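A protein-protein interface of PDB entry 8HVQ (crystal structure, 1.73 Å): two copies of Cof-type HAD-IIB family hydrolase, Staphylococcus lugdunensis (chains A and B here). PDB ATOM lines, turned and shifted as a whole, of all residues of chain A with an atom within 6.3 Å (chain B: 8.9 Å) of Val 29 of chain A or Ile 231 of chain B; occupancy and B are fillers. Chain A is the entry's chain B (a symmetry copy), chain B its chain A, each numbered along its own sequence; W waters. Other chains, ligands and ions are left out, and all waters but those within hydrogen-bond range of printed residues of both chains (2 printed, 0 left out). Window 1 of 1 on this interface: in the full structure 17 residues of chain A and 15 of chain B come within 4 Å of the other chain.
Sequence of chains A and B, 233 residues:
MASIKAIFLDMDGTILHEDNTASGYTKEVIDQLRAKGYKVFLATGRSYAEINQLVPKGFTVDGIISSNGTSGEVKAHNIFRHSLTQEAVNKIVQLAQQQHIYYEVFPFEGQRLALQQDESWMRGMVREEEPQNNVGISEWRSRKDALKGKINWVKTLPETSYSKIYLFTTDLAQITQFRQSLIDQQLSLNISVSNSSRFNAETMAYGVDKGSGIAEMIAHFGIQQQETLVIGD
Among the printed residues, merely in contact across the chains: Tyr 25 of chain A with Gly 232 of chain B, Gln 32 of chain A with Ile 231 of chain B, Lys 36 of chain A with Val 230 of chain B, Tyr 25 of chain A with Ile 15 of chain B, Lys 36 of chain A with Leu 229 of chain B, Tyr 25 of chain A with Asp 233 of chain B, Tyr 25 of chain A with Met 11 of chain B, Leu 33 of chain A with Ile 231 of chain B and Val 29 of chain A with Ile 231 of chain B.
O of Phe 8 of chain B is in hydrogen-bond range of N of Ile 231 of chain B (3.0 Å). O of Ala 43 of chain B lies within hydrogen-bond range of N of Met 11 of chain B, 3.1 Å away. The backbone NH of Asp 233 of chain B is in hydrogen-bond range of the backbone carbonyl oxygen of Asp 10 of chain B, 3.1 Å away. The backbone NH (N) of Leu 229 of chain B lies within hydrogen-bond range of the backbone carbonyl oxygen (O) of Ala 6 of chain B (2.8 Å). The backbone NH (N) of Asp 10 of chain B sits at hydrogen-bond distance from the backbone carbonyl oxygen (O) of Ile 231 of chain B. The backbone NH (N) of Phe 8 of chain B lies within hydrogen-bond range of the backbone carbonyl oxygen (O) of Leu 229 of chain B (2.8 Å).
Of the printed residues of chain B, Val 29 of chain A touches Ile 231. Printed residues of chain B within 4 Å of Gln 32 of chain A: Ile 231 (3.5 Å) and Gly 232 (2.6 Å). Of the printed residues of chain B, Lys 36 of chain A touches Leu 229 and Val 230. Of the printed residues of chain A, Ile 15 of chain B touches Tyr 25 (3.6 Å). Val 40 of chain B touches none of the printed residues of chain A. Lys 210 of chain B touches none of the printed residues of chain A. Printed residues of chain A within 4 Å of Leu 229 of chain B: Lys 36 (3.7 Å). Printed residues of chain A within 4 Å of Val 230 of chain B: Lys 36. Of the printed residues of chain A, Ile 231 of chain B touches Val 29, Gln 32 and Leu 33. The nearest printed residue of chain B that does not touch Val 29 of chain A is Gly 232 of chain B (4.4 Å).
The backbone NH (N) of Gly 232 of chain B lies within hydrogen-bond range of the side-chain amide oxygen (OE1) of Gln 32 of chain A (2.6 Å). OH of Tyr 25 of chain A lies within hydrogen-bond range of O of Asp 10 of chain B (2.7 Å).
Water W2 bridges NZ of Lys 36 of chain A (2.8 Å) and O of Val 230 of chain B (2.9 Å). Water W1 bridges N of Val 230 of chain B (2.9 Å) and NZ of Lys 36 of chain A (3.2 Å).
Positions printed for both chains: 26, 29 and 33.
Of the 23 printed residues of chain B, 8 touch a printed residue of chain A. Hydrophobic or aromatic side chains of chain B that line the printed part of chain A: Met 11, Ile 15, Leu 229 and Ile 231. Of the 12 printed residues of chain A, 5 touch a printed residue of chain B. Hydrophobic or aromatic side chains of chain A that line the printed part of chain B: Tyr 25, Val 29 and Leu 33. Among the printed residues, 11 pairs touch across the chains.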
ATOM      1  N   GLY A  24      -1.663  31.881  17.062  1.00  0.00           N
ATOM      2  CA  GLY A  24      -1.452  30.452  17.185  1.00  0.00           C
ATOM      3  C   GLY A  24      -0.420  30.131  18.258  1.00  0.00           C
ATOM      4  O   GLY A  24      -0.700  29.315  19.126  1.00  0.00           O
ATOM      5  N   TYR A  25       0.741  30.807  18.197  1.00  0.00           N
ATOM      6  CA  TYR A  25       1.827  30.536  19.122  1.00  0.00           C
ATOM      7  C   TYR A  25       1.387  30.876  20.544  1.00  0.00           C
ATOM      8  O   TYR A  25       1.677  30.116  21.464  1.00  0.00           O
ATOM      9  CB  TYR A  25       3.104  31.299  18.756  1.00  0.00           C
ATOM     10  CG  TYR A  25       4.344  30.914  19.548  1.00  0.00           C
ATOM     11  CD1 TYR A  25       5.014  29.722  19.309  1.00  0.00           C
ATOM     12  CD2 TYR A  25       4.865  31.747  20.526  1.00  0.00           C
ATOM     13  CE1 TYR A  25       6.156  29.363  20.017  1.00  0.00           C
ATOM     14  CE2 TYR A  25       6.002  31.405  21.256  1.00  0.00           C
ATOM     15  CZ  TYR A  25       6.666  30.211  21.000  1.00  0.00           C
ATOM     16  OH  TYR A  25       7.820  29.902  21.721  1.00  0.00           O
ATOM     17  N   THR A  26       0.698  32.015  20.706  1.00  0.00           N
ATOM     18  CA  THR A  26       0.276  32.476  22.023  1.00  0.00           C
ATOM     19  C   THR A  26      -0.739  31.508  22.624  1.00  0.00           C
ATOM     20  O   THR A  26      -0.651  31.120  23.791  1.00  0.00           O
ATOM     21  CB  THR A  26      -0.319  33.885  21.949  1.00  0.00           C
ATOM     22  OG1 THR A  26       0.615  34.726  21.280  1.00  0.00           O
ATOM     23  CG2 THR A  26      -0.605  34.464  23.313  1.00  0.00           C
ATOM     24  N   LYS A  27      -1.703  31.104  21.807  1.00  0.00           N
ATOM     25  CA  LYS A  27      -2.697  30.141  22.247  1.00  0.00           C
ATOM     26  C   LYS A  27      -2.007  28.845  22.667  1.00  0.00           C
ATOM     27  O   LYS A  27      -2.349  28.277  23.703  1.00  0.00           O
ATOM     28  CB  LYS A  27      -3.729  29.828  21.162  1.00  0.00           C
ATOM     29  CG  LYS A  27      -4.690  28.714  21.581  1.00  0.00           C
ATOM     30  CD  LYS A  27      -5.437  28.046  20.473  1.00  0.00           C
ATOM     31  CE  LYS A  27      -6.461  27.037  20.966  1.00  0.00           C
ATOM     32  NZ  LYS A  27      -5.862  25.710  21.260  1.00  0.00           N
ATOM     33  N   GLU A  28      -1.057  28.379  21.844  1.00  0.00           N
ATOM     34  CA  GLU A  28      -0.313  27.157  22.118  1.00  0.00           C
ATOM     35  C   GLU A  28       0.480  27.266  23.430  1.00  0.00           C
ATOM     36  O   GLU A  28       0.504  26.310  24.204  1.00  0.00           O
ATOM     37  CB  GLU A  28       0.649  26.849  20.968  1.00  0.00           C
ATOM     38  CG  GLU A  28      -0.043  26.585  19.636  1.00  0.00           C
ATOM     39  CD  GLU A  28      -0.142  25.134  19.189  1.00  0.00           C
ATOM     40  OE1 GLU A  28      -0.597  24.923  18.047  1.00  0.00           O
ATOM     41  OE2 GLU A  28       0.252  24.224  19.976  1.00  0.00           O
ATOM     42  N   VAL A  29       1.163  28.399  23.663  1.00  0.00           N
ATOM     43  CA  VAL A  29       1.919  28.588  24.893  1.00  0.00           C
ATOM     44  C   VAL A  29       0.985  28.554  26.111  1.00  0.00           C
ATOM     45  O   VAL A  29       1.267  27.865  27.098  1.00  0.00           O
ATOM     46  CB  VAL A  29       2.782  29.871  24.836  1.00  0.00           C
ATOM     47  CG1 VAL A  29       3.332  30.269  26.191  1.00  0.00           C
ATOM     48  CG2 VAL A  29       3.933  29.734  23.855  1.00  0.00           C
ATOM     49  N   ILE A  30      -0.164  29.244  26.018  1.00  0.00           N
ATOM     50  CA  ILE A  30      -1.111  29.269  27.120  1.00  0.00           C
ATOM     51  C   ILE A  30      -1.600  27.847  27.403  1.00  0.00           C
ATOM     52  O   ILE A  30      -1.619  27.440  28.551  1.00  0.00           O
ATOM     53  CB  ILE A  30      -2.254  30.271  26.867  1.00  0.00           C
ATOM     54  CG1 ILE A  30      -1.762  31.721  26.954  1.00  0.00           C
ATOM     55  CG2 ILE A  30      -3.390  30.027  27.834  1.00  0.00           C
ATOM     56  CD1 ILE A  30      -2.753  32.731  26.458  1.00  0.00           C
ATOM     57  N   ASP A  31      -1.926  27.074  26.361  1.00  0.00           N
ATOM     58  CA  ASP A  31      -2.387  25.700  26.529  1.00  0.00           C
ATOM     59  C   ASP A  31      -1.330  24.875  27.262  1.00  0.00           C
ATOM     60  O   ASP A  31      -1.641  24.090  28.143  1.00  0.00           O
ATOM     61  CB  ASP A  31      -2.702  24.996  25.198  1.00  0.00           C
ATOM     62  CG  ASP A  31      -3.883  25.500  24.381  1.00  0.00           C
ATOM     63  OD1 ASP A  31      -4.815  26.098  24.966  1.00  0.00           O
ATOM     64  OD2 ASP A  31      -3.861  25.275  23.142  1.00  0.00           O
ATOM     65  N   GLN A  32      -0.067  25.066  26.891  1.00  0.00           N
ATOM     66  CA  GLN A  32       1.036  24.350  27.508  1.00  0.00           C
ATOM     67  C   GLN A  32       1.168  24.690  28.987  1.00  0.00           C
ATOM     68  O   GLN A  32       1.282  23.798  29.827  1.00  0.00           O
ATOM     69  CB  GLN A  32       2.350  24.716  26.835  1.00  0.00           C
ATOM     70  CG  GLN A  32       2.688  23.812  25.681  1.00  0.00           C
ATOM     71  CD  GLN A  32       4.119  24.095  25.325  1.00  0.00           C
ATOM     72  OE1 GLN A  32       4.424  25.170  24.835  1.00  0.00           O
ATOM     73  NE2 GLN A  32       5.014  23.181  25.667  1.00  0.00           N
ATOM     74  N   LEU A  33       1.189  25.988  29.290  1.00  0.00           N
ATOM     75  CA  LEU A  33       1.280  26.451  30.671  1.00  0.00           C
ATOM     76  C   LEU A  33       0.142  25.849  31.495  1.00  0.00           C
ATOM     77  O   LEU A  33       0.341  25.373  32.609  1.00  0.00           O
ATOM     78  CB  LEU A  33       1.219  27.979  30.679  1.00  0.00           C
ATOM     79  CG  LEU A  33       2.441  28.696  30.110  1.00  0.00           C
ATOM     80  CD1 LEU A  33       2.197  30.189  29.989  1.00  0.00           C
ATOM     81  CD2 LEU A  33       3.655  28.430  30.969  1.00  0.00           C
ATOM     82  N   ARG A  34      -1.060  25.848  30.923  1.00  0.00           N
ATOM     83  CA  ARG A  34      -2.225  25.367  31.650  1.00  0.00           C
ATOM     84  C   ARG A  34      -2.119  23.860  31.846  1.00  0.00           C
ATOM     85  O   ARG A  34      -2.391  23.352  32.943  1.00  0.00           O
ATOM     86  CB  ARG A  34      -3.508  25.801  30.945  1.00  0.00           C
ATOM     87  CG  ARG A  34      -3.773  27.292  31.072  1.00  0.00           C
ATOM     88  CD  ARG A  34      -5.116  27.714  30.500  1.00  0.00           C
ATOM     89  NE  ARG A  34      -6.229  27.254  31.305  1.00  0.00           N
ATOM     90  CZ  ARG A  34      -7.124  26.316  30.972  1.00  0.00           C
ATOM     91  NH1 ARG A  34      -7.097  25.709  29.796  1.00  0.00           N
ATOM     92  NH2 ARG A  34      -8.059  25.983  31.840  1.00  0.00           N
ATOM     93  N   LYS A  36       0.565  22.286  32.176  1.00  0.00           N
ATOM     94  CA  LYS A  36       1.580  22.065  33.190  1.00  0.00           C
ATOM     95  C   LYS A  36       1.100  22.405  34.598  1.00  0.00           C
ATOM     96  O   LYS A  36       1.841  22.203  35.551  1.00  0.00           O
ATOM     97  CB  LYS A  36       2.809  22.917  32.858  1.00  0.00           C
ATOM     98  CG  LYS A  36       3.616  22.408  31.672  1.00  0.00           C
ATOM     99  CD  LYS A  36       4.696  23.356  31.202  1.00  0.00           C
ATOM    100  CE  LYS A  36       5.400  22.852  29.961  1.00  0.00           C
ATOM    101  NZ  LYS A  36       6.133  21.589  30.212  1.00  0.00           N
ATOM    102  N   ILE B   4      11.226  28.195  39.377  1.00  0.00           N
ATOM    103  CA  ILE B   4      11.766  28.201  38.035  1.00  0.00           C
ATOM    104  C   ILE B   4      12.785  29.318  38.003  1.00  0.00           C
ATOM    105  O   ILE B   4      12.449  30.424  38.399  1.00  0.00           O
ATOM    106  CB  ILE B   4      10.635  28.406  37.001  1.00  0.00           C
ATOM    107  CG1 ILE B   4       9.640  27.242  37.011  1.00  0.00           C
ATOM    108  CG2 ILE B   4      11.199  28.637  35.608  1.00  0.00           C
ATOM    109  CD1 ILE B   4      10.250  25.907  36.632  1.00  0.00           C
ATOM    110  N   ALA B   6      15.008  29.260  35.018  1.00  0.00           N
ATOM    111  CA  ALA B   6      15.261  29.346  33.586  1.00  0.00           C
ATOM    112  C   ALA B   6      13.979  29.050  32.814  1.00  0.00           C
ATOM    113  O   ALA B   6      13.261  28.106  33.167  1.00  0.00           O
ATOM    114  CB  ALA B   6      16.374  28.405  33.154  1.00  0.00           C
ATOM    115  N   ILE B   7      13.760  29.853  31.753  1.00  0.00           N
ATOM    116  CA  ILE B   7      12.680  29.681  30.802  1.00  0.00           C
ATOM    117  C   ILE B   7      13.291  29.537  29.409  1.00  0.00           C
ATOM    118  O   ILE B   7      14.063  30.408  28.977  1.00  0.00           O
ATOM    119  CB  ILE B   7      11.721  30.889  30.832  1.00  0.00           C
ATOM    120  CG1 ILE B   7      11.182  31.167  32.235  1.00  0.00           C
ATOM    121  CG2 ILE B   7      10.603  30.660  29.840  1.00  0.00           C
ATOM    122  CD1 ILE B   7      10.578  32.532  32.431  1.00  0.00           C
ATOM    123  N   PHE B   8      12.955  28.443  28.712  1.00  0.00           N
ATOM    124  CA  PHE B   8      13.323  28.279  27.310  1.00  0.00           C
ATOM    125  C   PHE B   8      12.115  28.503  26.409  1.00  0.00           C
ATOM    126  O   PHE B   8      11.090  27.876  26.627  1.00  0.00           O
ATOM    127  CB  PHE B   8      13.853  26.872  27.045  1.00  0.00           C
ATOM    128  CG  PHE B   8      15.303  26.704  27.372  1.00  0.00           C
ATOM    129  CD1 PHE B   8      16.267  26.846  26.386  1.00  0.00           C
ATOM    130  CD2 PHE B   8      15.693  26.397  28.667  1.00  0.00           C
ATOM    131  CE1 PHE B   8      17.604  26.713  26.709  1.00  0.00           C
ATOM    132  CE2 PHE B   8      17.024  26.270  28.983  1.00  0.00           C
ATOM    133  CZ  PHE B   8      17.971  26.405  28.003  1.00  0.00           C
ATOM    134  N   LEU B   9      12.227  29.382  25.409  1.00  0.00           N
ATOM    135  CA  LEU B   9      11.170  29.539  24.421  1.00  0.00           C
ATOM    136  C   LEU B   9      11.623  28.882  23.120  1.00  0.00           C
ATOM    137  O   LEU B   9      12.648  29.272  22.537  1.00  0.00           O
ATOM    138  CB  LEU B   9      10.855  31.024  24.216  1.00  0.00           C
ATOM    139  CG  LEU B   9      10.597  31.815  25.496  1.00  0.00           C
ATOM    140  CD1 LEU B   9      10.362  33.281  25.204  1.00  0.00           C
ATOM    141  CD2 LEU B   9       9.409  31.247  26.243  1.00  0.00           C
ATOM    142  N   ASP B  10      10.867  27.848  22.713  1.00  0.00           N
ATOM    143  CA  ASP B  10      11.139  27.146  21.479  1.00  0.00           C
ATOM    144  C   ASP B  10      10.327  27.816  20.378  1.00  0.00           C
ATOM    145  O   ASP B  10       9.113  27.955  20.471  1.00  0.00           O
ATOM    146  CB  ASP B  10      10.877  25.650  21.630  1.00  0.00           C
ATOM    147  CG  ASP B  10      11.372  24.830  20.451  1.00  0.00           C
ATOM    148  OD1 ASP B  10      11.289  25.335  19.328  1.00  0.00           O
ATOM    149  OD2 ASP B  10      11.824  23.688  20.666  1.00  0.00           O
ATOM    150  N   MET B  11      11.022  28.255  19.331  1.00  0.00           N
ATOM    151  CA  MET B  11      10.367  28.904  18.211  1.00  0.00           C
ATOM    152  C   MET B  11      11.272  28.851  16.980  1.00  0.00           C
ATOM    153  O   MET B  11      12.500  28.655  17.067  1.00  0.00           O
ATOM    154  CB  MET B  11      10.071  30.366  18.557  1.00  0.00           C
ATOM    155  CG  MET B  11      11.330  31.121  18.989  1.00  0.00           C
ATOM    156  SD  MET B  11      11.061  32.888  19.141  1.00  0.00           S
ATOM    157  CE  MET B  11       9.842  32.904  20.461  1.00  0.00           C
ATOM    158  N   ILE B  15       7.950  34.771  14.545  1.00  0.00           N
ATOM    159  CA  ILE B  15       7.154  35.588  15.459  1.00  0.00           C
ATOM    160  C   ILE B  15       7.866  36.907  15.781  1.00  0.00           C
ATOM    161  O   ILE B  15       7.228  37.899  16.138  1.00  0.00           O
ATOM    162  CB  ILE B  15       6.840  34.817  16.759  1.00  0.00           C
ATOM    163  CG1 ILE B  15       5.887  35.616  17.644  1.00  0.00           C
ATOM    164  CG2 ILE B  15       8.107  34.455  17.519  1.00  0.00           C
ATOM    165  CD1 ILE B  15       5.303  34.815  18.772  1.00  0.00           C
ATOM    166  N   THR B  26       6.676  40.193  22.261  1.00  0.00           N
ATOM    167  CA  THR B  26       7.496  39.062  22.655  1.00  0.00           C
ATOM    168  C   THR B  26       8.827  39.555  23.230  1.00  0.00           C
ATOM    169  O   THR B  26       9.293  39.071  24.269  1.00  0.00           O
ATOM    170  CB  THR B  26       7.739  38.121  21.470  1.00  0.00           C
ATOM    171  OG1 THR B  26       6.490  37.718  20.913  1.00  0.00           O
ATOM    172  CG2 THR B  26       8.542  36.895  21.857  1.00  0.00           C
ATOM    173  N   VAL B  29       8.016  41.034  26.660  1.00  0.00           N
ATOM    174  CA  VAL B  29       7.791  40.018  27.676  1.00  0.00           C
ATOM    175  C   VAL B  29       9.127  39.431  28.125  1.00  0.00           C
ATOM    176  O   VAL B  29       9.321  39.205  29.319  1.00  0.00           O
ATOM    177  CB  VAL B  29       6.825  38.905  27.218  1.00  0.00           C
ATOM    178  CG1 VAL B  29       6.824  37.741  28.195  1.00  0.00           C
ATOM    179  CG2 VAL B  29       5.413  39.422  27.024  1.00  0.00           C
ATOM    180  N   LEU B  33      10.619  39.472  31.988  1.00  0.00           N
ATOM    181  CA  LEU B  33      11.004  38.245  32.681  1.00  0.00           C
ATOM    182  C   LEU B  33      12.454  38.345  33.106  1.00  0.00           C
ATOM    183  O   LEU B  33      12.789  37.952  34.215  1.00  0.00           O
ATOM    184  CB  LEU B  33      10.835  37.026  31.778  1.00  0.00           C
ATOM    185  CG  LEU B  33       9.402  36.619  31.494  1.00  0.00           C
ATOM    186  CD1 LEU B  33       9.348  35.625  30.348  1.00  0.00           C
ATOM    187  CD2 LEU B  33       8.792  36.033  32.752  1.00  0.00           C
ATOM    188  N   VAL B  40      16.385  33.696  30.496  1.00  0.00           N
ATOM    189  CA  VAL B  40      15.506  33.367  29.396  1.00  0.00           C
ATOM    190  C   VAL B  40      16.371  32.986  28.211  1.00  0.00           C
ATOM    191  O   VAL B  40      17.365  33.662  27.909  1.00  0.00           O
ATOM    192  CB  VAL B  40      14.544  34.527  29.095  1.00  0.00           C
ATOM    193  CG1 VAL B  40      13.613  34.198  27.925  1.00  0.00           C
ATOM    194  CG2 VAL B  40      13.754  34.903  30.334  1.00  0.00           C
ATOM    195  N   PHE B  41      16.016  31.861  27.590  1.00  0.00           N
ATOM    196  CA  PHE B  41      16.790  31.278  26.503  1.00  0.00           C
ATOM    197  C   PHE B  41      15.875  31.051  25.302  1.00  0.00           C
ATOM    198  O   PHE B  41      14.688  30.793  25.488  1.00  0.00           O
ATOM    199  CB  PHE B  41      17.410  29.962  26.966  1.00  0.00           C
ATOM    200  CG  PHE B  41      18.315  30.107  28.160  1.00  0.00           C
ATOM    201  CD1 PHE B  41      19.629  30.498  28.017  1.00  0.00           C
ATOM    202  CD2 PHE B  41      17.843  29.861  29.440  1.00  0.00           C
ATOM    203  CE1 PHE B  41      20.467  30.643  29.113  1.00  0.00           C
ATOM    204  CE2 PHE B  41      18.675  30.026  30.530  1.00  0.00           C
ATOM    205  CZ  PHE B  41      19.989  30.433  30.358  1.00  0.00           C
ATOM    206  N   LEU B  42      16.416  31.177  24.087  1.00  0.00           N
ATOM    207  CA  LEU B  42      15.743  30.614  22.922  1.00  0.00           C
ATOM    208  C   LEU B  42      16.276  29.225  22.607  1.00  0.00           C
ATOM    209  O   LEU B  42      17.478  28.983  22.660  1.00  0.00           O
ATOM    210  CB  LEU B  42      15.996  31.449  21.672  1.00  0.00           C
ATOM    211  CG  LEU B  42      15.470  32.873  21.655  1.00  0.00           C
ATOM    212  CD1 LEU B  42      15.667  33.461  20.262  1.00  0.00           C
ATOM    213  CD2 LEU B  42      14.007  32.919  22.053  1.00  0.00           C
ATOM    214  N   ALA B  43      15.382  28.384  22.098  1.00  0.00           N
ATOM    215  CA  ALA B  43      15.752  27.149  21.435  1.00  0.00           C
ATOM    216  C   ALA B  43      15.143  27.175  20.044  1.00  0.00           C
ATOM    217  O   ALA B  43      13.950  27.511  19.881  1.00  0.00           O
ATOM    218  CB  ALA B  43      15.256  25.970  22.222  1.00  0.00           C
ATOM    219  N   LYS B 210      17.529  18.790  21.081  1.00  0.00           N
ATOM    220  CA  LYS B 210      17.165  20.012  21.777  1.00  0.00           C
ATOM    221  C   LYS B 210      17.321  19.827  23.278  1.00  0.00           C
ATOM    222  O   LYS B 210      17.744  20.746  23.961  1.00  0.00           O
ATOM    223  CB  LYS B 210      15.766  20.489  21.408  1.00  0.00           C
ATOM    224  CG  LYS B 210      15.740  21.262  20.093  1.00  0.00           C
ATOM    225  CD  LYS B 210      14.415  21.911  19.881  1.00  0.00           C
ATOM    226  CE  LYS B 210      14.342  22.674  18.581  1.00  0.00           C
ATOM    227  NZ  LYS B 210      12.932  22.874  18.193  1.00  0.00           N
ATOM    228  N   ILE B 214      19.540  22.016  25.869  1.00  0.00           N
ATOM    229  CA  ILE B 214      18.951  22.653  27.026  1.00  0.00           C
ATOM    230  C   ILE B 214      19.773  22.282  28.253  1.00  0.00           C
ATOM    231  O   ILE B 214      20.086  23.146  29.072  1.00  0.00           O
ATOM    232  CB  ILE B 214      17.463  22.255  27.149  1.00  0.00           C
ATOM    233  CG1 ILE B 214      16.625  22.973  26.086  1.00  0.00           C
ATOM    234  CG2 ILE B 214      16.953  22.567  28.541  1.00  0.00           C
ATOM    235  CD1 ILE B 214      15.254  22.370  25.874  1.00  0.00           C
ATOM    236  N   THR B 228      13.857  24.463  35.405  1.00  0.00           N
ATOM    237  CA  THR B 228      13.745  24.925  34.025  1.00  0.00           C
ATOM    238  C   THR B 228      12.348  24.704  33.467  1.00  0.00           C
ATOM    239  O   THR B 228      11.803  23.603  33.564  1.00  0.00           O
ATOM    240  CB  THR B 228      14.820  24.240  33.175  1.00  0.00           C
ATOM    241  OG1 THR B 228      16.076  24.519  33.811  1.00  0.00           O
ATOM    242  CG2 THR B 228      14.806  24.705  31.730  1.00  0.00           C
ATOM    243  N   LEU B 229      11.782  25.749  32.850  1.00  0.00           N
ATOM    244  CA  LEU B 229      10.504  25.617  32.154  1.00  0.00           C
ATOM    245  C   LEU B 229      10.750  25.755  30.654  1.00  0.00           C
ATOM    246  O   LEU B 229      11.431  26.686  30.228  1.00  0.00           O
ATOM    247  CB  LEU B 229       9.568  26.712  32.671  1.00  0.00           C
ATOM    248  CG  LEU B 229       8.259  26.900  31.921  1.00  0.00           C
ATOM    249  CD1 LEU B 229       7.280  25.786  32.276  1.00  0.00           C
ATOM    250  CD2 LEU B 229       7.662  28.278  32.213  1.00  0.00           C
ATOM    251  N   VAL B 230      10.182  24.823  29.881  1.00  0.00           N
ATOM    252  CA  VAL B 230      10.355  24.764  28.440  1.00  0.00           C
ATOM    253  C   VAL B 230       8.982  24.892  27.797  1.00  0.00           C
ATOM    254  O   VAL B 230       8.141  24.016  28.022  1.00  0.00           O
ATOM    255  CB  VAL B 230      11.033  23.441  28.050  1.00  0.00           C
ATOM    256  CG1 VAL B 230      11.227  23.337  26.548  1.00  0.00           C
ATOM    257  CG2 VAL B 230      12.357  23.249  28.771  1.00  0.00           C
ATOM    258  N   ILE B 231       8.773  25.948  26.992  1.00  0.00           N
ATOM    259  CA  ILE B 231       7.488  26.179  26.339  1.00  0.00           C
ATOM    260  C   ILE B 231       7.704  26.517  24.861  1.00  0.00           C
ATOM    261  O   ILE B 231       8.791  26.940  24.466  1.00  0.00           O
ATOM    262  CB  ILE B 231       6.680  27.260  27.085  1.00  0.00           C
ATOM    263  CG1 ILE B 231       7.453  28.565  27.280  1.00  0.00           C
ATOM    264  CG2 ILE B 231       6.190  26.720  28.415  1.00  0.00           C
ATOM    265  CD1 ILE B 231       6.748  29.591  28.146  1.00  0.00           C
ATOM    266  N   GLY B 232       6.670  26.324  24.033  1.00  0.00           N
ATOM    267  CA  GLY B 232       6.752  26.641  22.608  1.00  0.00           C
ATOM    268  C   GLY B 232       6.643  25.395  21.723  1.00  0.00           C
ATOM    269  O   GLY B 232       6.087  24.378  22.138  1.00  0.00           O
ATOM    270  N   ASP B 233       7.142  25.513  20.485  1.00  0.00           N
ATOM    271  CA  ASP B 233       7.272  24.404  19.545  1.00  0.00           C
ATOM    272  C   ASP B 233       8.098  23.279  20.190  1.00  0.00           C
ATOM    273  O   ASP B 233       7.482  22.296  20.659  1.00  0.00           O
ATOM    274  CB  ASP B 233       7.949  24.850  18.236  1.00  0.00           C
ATOM    275  CG  ASP B 233       7.300  26.014  17.495  1.00  0.00           C
ATOM    276  OD1 ASP B 233       6.134  26.320  17.799  1.00  0.00           O
ATOM    277  OD2 ASP B 233       7.973  26.611  16.611  1.00  0.00           O
HETATM  278  O   HOH W   1       9.074  22.442  31.073  1.00  0.00           O
HETATM  279  O   HOH W   2       7.901  21.092  28.033  1.00  0.00           O
